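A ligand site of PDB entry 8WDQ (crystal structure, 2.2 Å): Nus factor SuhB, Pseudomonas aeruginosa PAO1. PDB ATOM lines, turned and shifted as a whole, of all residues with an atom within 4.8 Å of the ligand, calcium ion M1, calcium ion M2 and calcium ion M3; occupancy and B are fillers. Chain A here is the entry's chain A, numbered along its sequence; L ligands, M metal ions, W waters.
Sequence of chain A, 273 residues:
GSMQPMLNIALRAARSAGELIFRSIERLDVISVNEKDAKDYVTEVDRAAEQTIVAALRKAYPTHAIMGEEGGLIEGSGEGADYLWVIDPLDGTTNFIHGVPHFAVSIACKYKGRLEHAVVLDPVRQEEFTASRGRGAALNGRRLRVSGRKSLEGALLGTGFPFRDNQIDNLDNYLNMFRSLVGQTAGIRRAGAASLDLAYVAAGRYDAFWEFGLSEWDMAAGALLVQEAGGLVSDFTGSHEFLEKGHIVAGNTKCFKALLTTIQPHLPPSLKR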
ATOM      1  N   LYS A  36      -7.411  -4.960 -10.479  1.00  0.00           N
ATOM      2  CA  LYS A  36      -7.180  -6.039 -11.426  1.00  0.00           C
ATOM      3  C   LYS A  36      -8.243  -7.123 -11.274  1.00  0.00           C
ATOM      4  O   LYS A  36      -8.837  -7.578 -12.263  1.00  0.00           O
ATOM      5  CB  LYS A  36      -5.779  -6.628 -11.219  1.00  0.00           C
ATOM      6  CG  LYS A  36      -4.644  -5.700 -11.652  1.00  0.00           C
ATOM      7  CD  LYS A  36      -3.293  -6.402 -11.568  1.00  0.00           C
ATOM      8  CE  LYS A  36      -3.025  -6.921 -10.170  1.00  0.00           C
ATOM      9  NZ  LYS A  36      -1.687  -7.573 -10.065  1.00  0.00           N
ATOM     10  N   ASP A  40      -8.152  -7.437  -5.513  1.00  0.00           N
ATOM     11  CA  ASP A  40      -6.813  -7.453  -6.089  1.00  0.00           C
ATOM     12  C   ASP A  40      -6.542  -6.055  -6.627  1.00  0.00           C
ATOM     13  O   ASP A  40      -7.028  -5.690  -7.706  1.00  0.00           O
ATOM     14  CB  ASP A  40      -6.712  -8.515  -7.170  1.00  0.00           C
ATOM     15  CG  ASP A  40      -5.280  -8.824  -7.578  1.00  0.00           C
ATOM     16  OD1 ASP A  40      -4.404  -8.822  -6.694  1.00  0.00           O
ATOM     17  OD2 ASP A  40      -5.043  -9.069  -8.780  1.00  0.00           O
ATOM     18  N   ASP A  46       2.592   0.528  -7.487  1.00  0.00           N
ATOM     19  CA  ASP A  46       3.007  -0.785  -7.967  1.00  0.00           C
ATOM     20  C   ASP A  46       3.687  -0.688  -9.331  1.00  0.00           C
ATOM     21  O   ASP A  46       4.758  -1.269  -9.546  1.00  0.00           O
ATOM     22  CB  ASP A  46       1.802  -1.738  -8.044  1.00  0.00           C
ATOM     23  CG  ASP A  46       1.130  -1.951  -6.697  1.00  0.00           C
ATOM     24  OD1 ASP A  46       1.592  -2.802  -5.913  1.00  0.00           O
ATOM     25  OD2 ASP A  46       0.113  -1.279  -6.437  1.00  0.00           O
ATOM     26  N   GLU A  69       4.667  -8.847 -11.740  1.00  0.00           N
ATOM     27  CA  GLU A  69       3.246  -8.993 -11.412  1.00  0.00           C
ATOM     28  C   GLU A  69       2.392  -8.095 -12.306  1.00  0.00           C
ATOM     29  O   GLU A  69       1.383  -8.540 -12.863  1.00  0.00           O
ATOM     30  CB  GLU A  69       2.994  -8.688  -9.939  1.00  0.00           C
ATOM     31  CG  GLU A  69       1.539  -8.352  -9.656  1.00  0.00           C
ATOM     32  CD  GLU A  69       1.125  -8.528  -8.205  1.00  0.00           C
ATOM     33  OE1 GLU A  69       1.988  -8.423  -7.295  1.00  0.00           O
ATOM     34  OE2 GLU A  69      -0.078  -8.777  -7.968  1.00  0.00           O
ATOM     35  N   GLU A  70       2.791  -6.842 -12.474  1.00  0.00           N
ATOM     36  CA  GLU A  70       1.994  -5.928 -13.302  1.00  0.00           C
ATOM     37  C   GLU A  70       2.224  -6.167 -14.790  1.00  0.00           C
ATOM     38  O   GLU A  70       1.265  -6.142 -15.574  1.00  0.00           O
ATOM     39  CB  GLU A  70       2.292  -4.477 -12.945  1.00  0.00           C
ATOM     40  CG  GLU A  70       2.327  -4.152 -11.444  1.00  0.00           C
ATOM     41  CD  GLU A  70       1.158  -4.748 -10.667  1.00  0.00           C
ATOM     42  OE1 GLU A  70       0.045  -4.883 -11.223  1.00  0.00           O
ATOM     43  OE2 GLU A  70       1.355  -5.076  -9.467  1.00  0.00           O
ATOM     44  N   ASP A  88       7.656  -9.221  -7.589  1.00  0.00           N
ATOM     45  CA  ASP A  88       6.523  -8.530  -6.997  1.00  0.00           C
ATOM     46  C   ASP A  88       7.021  -7.151  -6.590  1.00  0.00           C
ATOM     47  O   ASP A  88       7.740  -7.027  -5.588  1.00  0.00           O
ATOM     48  CB  ASP A  88       5.959  -9.269  -5.788  1.00  0.00           C
ATOM     49  CG  ASP A  88       4.592  -8.734  -5.367  1.00  0.00           C
ATOM     50  OD1 ASP A  88       4.282  -7.571  -5.695  1.00  0.00           O
ATOM     51  OD2 ASP A  88       3.864  -9.458  -4.669  1.00  0.00           O
ATOM     52  N   LEU A  90       5.532  -4.677  -5.202  1.00  0.00           N
ATOM     53  CA  LEU A  90       4.984  -4.226  -3.926  1.00  0.00           C
ATOM     54  C   LEU A  90       4.105  -5.358  -3.395  1.00  0.00           C
ATOM     55  O   LEU A  90       2.954  -5.514  -3.813  1.00  0.00           O
ATOM     56  CB  LEU A  90       4.197  -2.941  -4.095  1.00  0.00           C
ATOM     57  CG  LEU A  90       3.395  -2.392  -2.902  1.00  0.00           C
ATOM     58  CD1 LEU A  90       4.199  -2.436  -1.608  1.00  0.00           C
ATOM     59  CD2 LEU A  90       2.924  -0.982  -3.192  1.00  0.00           C
ATOM     60  N   ASP A  91       4.654  -6.157  -2.490  1.00  0.00           N
ATOM     61  CA  ASP A  91       3.889  -7.228  -1.848  1.00  0.00           C
ATOM     62  C   ASP A  91       3.353  -6.732  -0.504  1.00  0.00           C
ATOM     63  O   ASP A  91       4.127  -6.308   0.353  1.00  0.00           O
ATOM     64  CB  ASP A  91       4.739  -8.492  -1.729  1.00  0.00           C
ATOM     65  CG  ASP A  91       4.028  -9.628  -1.014  1.00  0.00           C
ATOM     66  OD1 ASP A  91       4.627 -10.219  -0.124  1.00  0.00           O
ATOM     67  OD2 ASP A  91       2.832  -9.855  -1.204  1.00  0.00           O
ATOM     68  N   GLY A  92       2.033  -6.761  -0.359  1.00  0.00           N
ATOM     69  CA  GLY A  92       1.331  -6.109   0.732  1.00  0.00           C
ATOM     70  C   GLY A  92       0.548  -4.871   0.293  1.00  0.00           C
ATOM     71  O   GLY A  92       0.524  -3.862   1.008  1.00  0.00           O
ATOM     72  N   THR A  93      -0.113  -4.957  -0.874  1.00  0.00           N
ATOM     73  CA  THR A  93      -0.747  -3.783  -1.484  1.00  0.00           C
ATOM     74  C   THR A  93      -1.913  -3.269  -0.653  1.00  0.00           C
ATOM     75  O   THR A  93      -2.137  -2.052  -0.565  1.00  0.00           O
ATOM     76  CB  THR A  93      -1.206  -4.127  -2.908  1.00  0.00           C
ATOM     77  OG1 THR A  93      -0.057  -4.355  -3.749  1.00  0.00           O
ATOM     78  CG2 THR A  93      -2.023  -3.001  -3.505  1.00  0.00           C
ATOM     79  N   THR A  94      -2.701  -4.157  -0.037  1.00  0.00           N
ATOM     80  CA  THR A  94      -3.819  -3.699   0.774  1.00  0.00           C
ATOM     81  C   THR A  94      -3.331  -2.986   2.030  1.00  0.00           C
ATOM     82  O   THR A  94      -3.835  -1.913   2.388  1.00  0.00           O
ATOM     83  CB  THR A  94      -4.734  -4.881   1.107  1.00  0.00           C
ATOM     84  OG1 THR A  94      -5.102  -5.544  -0.113  1.00  0.00           O
ATOM     85  CG2 THR A  94      -5.998  -4.415   1.839  1.00  0.00           C
ATOM     86  N   GLY A 160      -1.632 -16.811   5.716  1.00  0.00           N
ATOM     87  CA  GLY A 160      -2.404 -15.870   4.914  1.00  0.00           C
ATOM     88  C   GLY A 160      -3.821 -16.357   4.756  1.00  0.00           C
ATOM     89  O   GLY A 160      -4.060 -17.551   4.572  1.00  0.00           O
ATOM     90  N   PHE A 161      -4.765 -15.420   4.815  1.00  0.00           N
ATOM     91  CA  PHE A 161      -6.184 -15.752   4.834  1.00  0.00           C
ATOM     92  C   PHE A 161      -6.722 -15.920   3.425  1.00  0.00           C
ATOM     93  O   PHE A 161      -6.367 -15.156   2.525  1.00  0.00           O
ATOM     94  CB  PHE A 161      -6.989 -14.663   5.563  1.00  0.00           C
ATOM     95  CG  PHE A 161      -6.647 -14.517   7.008  1.00  0.00           C
ATOM     96  CD1 PHE A 161      -6.165 -15.595   7.744  1.00  0.00           C
ATOM     97  CD2 PHE A 161      -6.822 -13.289   7.649  1.00  0.00           C
ATOM     98  CE1 PHE A 161      -5.858 -15.449   9.081  1.00  0.00           C
ATOM     99  CE2 PHE A 161      -6.511 -13.148   8.993  1.00  0.00           C
ATOM    100  CZ  PHE A 161      -6.040 -14.226   9.711  1.00  0.00           C
ATOM    101  N   PHE A 163      -8.995 -14.825   1.312  1.00  0.00           N
ATOM    102  CA  PHE A 163      -9.893 -13.667   1.327  1.00  0.00           C
ATOM    103  C   PHE A 163     -10.630 -13.445   0.004  1.00  0.00           C
ATOM    104  O   PHE A 163     -11.594 -12.684  -0.010  1.00  0.00           O
ATOM    105  CB  PHE A 163      -9.107 -12.402   1.688  1.00  0.00           C
ATOM    106  CG  PHE A 163      -8.061 -12.029   0.665  1.00  0.00           C
ATOM    107  CD1 PHE A 163      -6.814 -12.617   0.691  1.00  0.00           C
ATOM    108  CD2 PHE A 163      -8.336 -11.074  -0.309  1.00  0.00           C
ATOM    109  CE1 PHE A 163      -5.848 -12.266  -0.247  1.00  0.00           C
ATOM    110  CE2 PHE A 163      -7.384 -10.728  -1.255  1.00  0.00           C
ATOM    111  CZ  PHE A 163      -6.132 -11.321  -1.221  1.00  0.00           C
ATOM    112  N   ARG A 164     -10.200 -14.068  -1.083  1.00  0.00           N
ATOM    113  CA  ARG A 164     -10.800 -13.828  -2.384  1.00  0.00           C
ATOM    114  C   ARG A 164     -12.165 -14.497  -2.481  1.00  0.00           C
ATOM    115  O   ARG A 164     -12.439 -15.498  -1.810  1.00  0.00           O
ATOM    116  CB  ARG A 164      -9.894 -14.328  -3.507  1.00  0.00           C
ATOM    117  CG  ARG A 164      -8.532 -13.649  -3.581  1.00  0.00           C
ATOM    118  CD  ARG A 164      -7.544 -14.502  -4.372  1.00  0.00           C
ATOM    119  NE  ARG A 164      -6.177 -13.985  -4.284  1.00  0.00           N
ATOM    120  CZ  ARG A 164      -5.349 -14.196  -3.274  1.00  0.00           C
ATOM    121  NH1 ARG A 164      -5.709 -14.944  -2.235  1.00  0.00           N
ATOM    122  NH2 ARG A 164      -4.129 -13.662  -3.310  1.00  0.00           N
ATOM    123  N   ARG A 190      -1.077 -13.024  10.952  1.00  0.00           N
ATOM    124  CA  ARG A 190      -1.431 -12.706   9.568  1.00  0.00           C
ATOM    125  C   ARG A 190      -1.131 -11.224   9.405  1.00  0.00           C
ATOM    126  O   ARG A 190      -1.989 -10.370   9.637  1.00  0.00           O
ATOM    127  CB  ARG A 190      -2.889 -13.041   9.262  1.00  0.00           C
ATOM    128  CG  ARG A 190      -3.191 -13.194   7.765  1.00  0.00           C
ATOM    129  CD  ARG A 190      -3.455 -11.843   7.096  1.00  0.00           C
ATOM    130  NE  ARG A 190      -4.042 -11.983   5.767  1.00  0.00           N
ATOM    131  CZ  ARG A 190      -3.361 -12.259   4.667  1.00  0.00           C
ATOM    132  NH1 ARG A 190      -2.052 -12.461   4.695  1.00  0.00           N
ATOM    133  NH2 ARG A 190      -4.001 -12.326   3.499  1.00  0.00           N
ATOM    134  N   GLY A 192       0.054  -9.760   6.522  1.00  0.00           N
ATOM    135  CA  GLY A 192      -0.421  -9.287   5.242  1.00  0.00           C
ATOM    136  C   GLY A 192       0.602  -9.129   4.138  1.00  0.00           C
ATOM    137  O   GLY A 192       0.328  -8.398   3.167  1.00  0.00           O
ATOM    138  N   ALA A 193       1.757  -9.780   4.220  1.00  0.00           N
ATOM    139  CA  ALA A 193       2.733  -9.749   3.124  1.00  0.00           C
ATOM    140  C   ALA A 193       3.459 -11.088   3.092  1.00  0.00           C
ATOM    141  O   ALA A 193       4.344 -11.336   3.908  1.00  0.00           O
ATOM    142  CB  ALA A 193       3.709  -8.586   3.281  1.00  0.00           C
ATOM    143  N   ALA A 194       3.099 -11.933   2.124  1.00  0.00           N
ATOM    144  CA  ALA A 194       3.593 -13.309   2.101  1.00  0.00           C
ATOM    145  C   ALA A 194       5.113 -13.375   1.982  1.00  0.00           C
ATOM    146  O   ALA A 194       5.744 -14.271   2.569  1.00  0.00           O
ATOM    147  CB  ALA A 194       2.931 -14.084   0.960  1.00  0.00           C
ATOM    148  N   SER A 195       5.714 -12.471   1.213  1.00  0.00           N
ATOM    149  CA  SER A 195       7.169 -12.486   1.083  1.00  0.00           C
ATOM    150  C   SER A 195       7.839 -12.259   2.425  1.00  0.00           C
ATOM    151  O   SER A 195       8.867 -12.877   2.738  1.00  0.00           O
ATOM    152  CB  SER A 195       7.643 -11.438   0.069  1.00  0.00           C
ATOM    153  OG  SER A 195       7.271 -10.137   0.480  1.00  0.00           O
ATOM    154  N   GLU A 211      -0.150 -21.234   3.287  1.00  0.00           N
ATOM    155  CA  GLU A 211      -1.120 -20.391   2.594  1.00  0.00           C
ATOM    156  C   GLU A 211      -1.416 -21.020   1.238  1.00  0.00           C
ATOM    157  O   GLU A 211      -0.526 -21.609   0.624  1.00  0.00           O
ATOM    158  CB  GLU A 211      -0.607 -18.950   2.403  1.00  0.00           C
ATOM    159  CG  GLU A 211      -1.595 -18.036   1.683  1.00  0.00           C
ATOM    160  CD  GLU A 211      -1.231 -16.554   1.765  1.00  0.00           C
ATOM    161  OE1 GLU A 211      -0.136 -16.221   2.261  1.00  0.00           O
ATOM    162  OE2 GLU A 211      -2.055 -15.716   1.343  1.00  0.00           O
ATOM    163  N   LEU A 214      -1.682 -18.289  -3.655  1.00  0.00           N
ATOM    164  CA  LEU A 214      -0.603 -17.352  -3.936  1.00  0.00           C
ATOM    165  C   LEU A 214      -0.140 -17.465  -5.384  1.00  0.00           C
ATOM    166  O   LEU A 214      -0.364 -18.471  -6.072  1.00  0.00           O
ATOM    167  CB  LEU A 214       0.594 -17.610  -3.008  1.00  0.00           C
ATOM    168  CG  LEU A 214       0.426 -17.229  -1.540  1.00  0.00           C
ATOM    169  CD1 LEU A 214       1.688 -17.604  -0.752  1.00  0.00           C
ATOM    170  CD2 LEU A 214       0.120 -15.744  -1.371  1.00  0.00           C
ATOM    171  N   ASP A 218       4.727 -13.934  -5.385  1.00  0.00           N
ATOM    172  CA  ASP A 218       4.564 -13.858  -3.935  1.00  0.00           C
ATOM    173  C   ASP A 218       5.579 -14.739  -3.226  1.00  0.00           C
ATOM    174  O   ASP A 218       6.054 -14.396  -2.130  1.00  0.00           O
ATOM    175  CB  ASP A 218       3.145 -14.286  -3.524  1.00  0.00           C
ATOM    176  CG  ASP A 218       2.055 -13.445  -4.163  1.00  0.00           C
ATOM    177  OD1 ASP A 218       2.146 -12.196  -4.184  1.00  0.00           O
ATOM    178  OD2 ASP A 218       1.083 -14.054  -4.666  1.00  0.00           O
HETATM  179  C1  LIG L   1      -0.099 -11.079  -1.488  1.00  0.00           C
HETATM  180  C2  LIG L   1       0.162 -10.618  -0.040  1.00  0.00           C
HETATM  181  C3  LIG L   1      -0.776 -11.171   1.039  1.00  0.00           C
HETATM  182  C4  LIG L   1      -1.310 -12.542   0.630  1.00  0.00           C
HETATM  183  C5  LIG L   1      -2.178 -12.402  -0.626  1.00  0.00           C
HETATM  184  C6  LIG L   1      -1.390 -11.850  -1.837  1.00  0.00           C
HETATM  185  P1  LIG L   1      -0.208  -8.620  -2.894  1.00  0.00           P
HETATM  186  O1  LIG L   1       0.322 -10.128  -2.461  1.00  0.00           O
HETATM  187  O2  LIG L   1       1.421 -11.200   0.239  1.00  0.00           O
HETATM  188  O3  LIG L   1      -0.049 -11.316   2.245  1.00  0.00           O
HETATM  189  O4  LIG L   1      -2.081 -13.083   1.685  1.00  0.00           O
HETATM  190  O5  LIG L   1      -2.642 -13.686  -0.962  1.00  0.00           O
HETATM  191  O6  LIG L   1      -2.220 -11.081  -2.676  1.00  0.00           O
HETATM  192  O7  LIG L   1      -0.161  -7.624  -1.754  1.00  0.00           O
HETATM  193  O8  LIG L   1       0.784  -8.199  -3.949  1.00  0.00           O
HETATM  194  O9  LIG L   1      -1.592  -8.650  -3.519  1.00  0.00           O
HETATM  195 CA    CA M   1       2.661 -10.215  -2.940  1.00  0.00          CA
HETATM  196 CA    CA M   2       2.106  -6.978  -5.398  1.00  0.00          CA
HETATM  197 CA    CA M   3      -1.220  -8.679  -5.864  1.00  0.00          CA
HETATM  198  O   HOH W   1      -4.576 -15.934   0.492  1.00  0.00           O
HETATM  199  O   HOH W   2       0.615 -13.783   3.497  1.00  0.00           O
HETATM  200  O   HOH W   3      -1.348 -13.113  -5.064  1.00  0.00           O
HETATM  201  O   HOH W   4      -2.215  -7.122  -0.083  1.00  0.00           O
HETATM  202  O   HOH W   5      -5.003 -10.368  -4.355  1.00  0.00           O
HETATM  203  O   HOH W   6      -3.017  -7.055  -6.127  1.00  0.00           O
HETATM  204  O   HOH W   7      -3.912  -8.698  -2.743  1.00  0.00           O
HETATM  205  O   HOH W   8      -0.297  -6.301  -5.640  1.00  0.00           O
HETATM  206  O   HOH W   9       2.163  -5.071  -6.859  1.00  0.00           O
HETATM  207  O   HOH W  10       0.216 -10.691  -5.944  1.00  0.00           O
HETATM  208  O   HOH W  11      -2.867 -10.486  -6.178  1.00  0.00           O
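The side-chain carboxylate (OD2) of Asp 91 binds calcium ion M1 (1.8 Å).
The side-chain carboxylate (OD2) of Asp 88 binds calcium ion M1.
O1 of the ligand binds calcium ion M1.
OD1 of Asp 218 is bound to calcium ion M1.
Slightly farther from calcium ion M1 lies an oxygen (O8) of the ligand (2.9 Å).
OE2 of Glu 211 is in hydrogen-bond range of O4 of the ligand (2.7 Å).
O5 of the ligand is in hydrogen-bond range of NH2 of Arg 164, at 2.8 Å.
An oxygen (O4) of the ligand lies within hydrogen-bond range of the guanidinium group (NH2) of Arg 190.
O3 of the ligand is in hydrogen-bond range of N of Ala 193.
O7 of the ligand lies within hydrogen-bond range of N of Thr 93, at 2.8 Å.
The backbone NH of Ala 194 lies within hydrogen-bond range of an oxygen (O2) of the ligand (2.6 Å).
O7 of the ligand sits at hydrogen-bond distance from N of Gly 92.
An oxygen (O3) of the ligand sits close to the backbone carbonyl oxygen (O) of Gly 192 (3.1 Å).
Thr 93 touches calcium ion M2 (OG1 to CA, 3.8 Å).
Five residues have an atom within 4 Å of calcium ion M2: Glu 69, Asp 88, Leu 90, Asp 91 and Thr 93.
The side-chain carboxylate (OD1) of Asp 91 sits at hydrogen-bond distance from the backbone NH (N) of Ala 194 (3.2 Å).
The side-chain hydroxyl of Thr 93 lies close to the backbone carbonyl oxygen of Leu 90 (3.2 Å).
OG1 of Thr 93 sits at hydrogen-bond distance from OD1 of Asp 46.
The side-chain amino group (NZ) of Lys 36 lies within salt-bridge range of the side-chain carboxylate (OD2) of Asp 40 (3.9 Å).
The side-chain carboxylate (OD1) of Asp 91 sits at hydrogen-bond distance from the side-chain hydroxyl (OG) of Ser 195, at 2.7 Å.
The side-chain carboxylate of Glu 69 lies close to the side-chain amino group of Lys 36 (2.9 Å).
Calcium ion M3 is bound by O9 of the ligand (2.4 Å), OE2 of Glu 69 (2.4 Å), water W6 (2.4 Å), water W11 (2.5 Å), water W10 (2.5 Å), water W8 (2.6 Å) and O8 of the ligand (2.8 Å).
Calcium ion M3 has seven donor atoms within binding distance.
Merely in contact with the ligand: Leu 214 (3.5 Å) and Phe 163 (3.6 Å).
15 residues have an atom within 4 Å of the ligand: Glu 69, Asp 88, Leu 90, Asp 91, Gly 92, Thr 93, Phe 163, Arg 164, Arg 190, Gly 192, Ala 193, Ala 194, Glu 211, Leu 214 and Asp 218.
Residues that only touch calcium ion M3: Asp 40 (3.3 Å).
Within 4 Å of calcium ion M3: Asp 40 and Glu 69.
The side-chain carboxylate (OD1) of Asp 88 is bound to calcium ion M2 (2.3 Å).
Calcium ion M2 is bound by O8 of the ligand (2.3 Å).
The backbone carbonyl oxygen (O) of Leu 90 is bound to calcium ion M2 (2.3 Å).
OE1 of Glu 69 binds calcium ion M2, 2.4 Å away.
Water W9 binds calcium ion M2 (2.4 Å).
Water W8 is bound to calcium ion M2 (2.5 Å).
Slightly farther from calcium ion M2 lies OD2 of Asp 88 (3.1 Å).
Water W9 lies within hydrogen-bond range of OD1 of Asp 46 and OE2 of Glu 70.
Water W4 lies within hydrogen-bond range of an oxygen (O7) of the ligand (2.7 Å), the backbone NH of Thr 94 (3.0 Å) and the backbone NH of Thr 93 (3.1 Å).
Water W2 lies within hydrogen-bond range of OE1 of Glu 211 (2.8 Å), O3 of the ligand (2.8 Å), NH1 of Arg 190 (3.2 Å) and N of Ala 194 (3.4 Å).
Water W3 lies within hydrogen-bond range of OD2 of Asp 218 (2.6 Å), O6 of the ligand (3.3 Å) and NH2 of Arg 164 (3.3 Å).
Water W1 lies within hydrogen-bond range of OE2 of Glu 211, O of Phe 161, NH1 of Arg 164 and O5 of the ligand.
Water W5 lies within hydrogen-bond range of the side-chain carboxylate (OD1) of Asp 40 (2.9 Å) and an oxygen (O6) of the ligand (3.3 Å).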
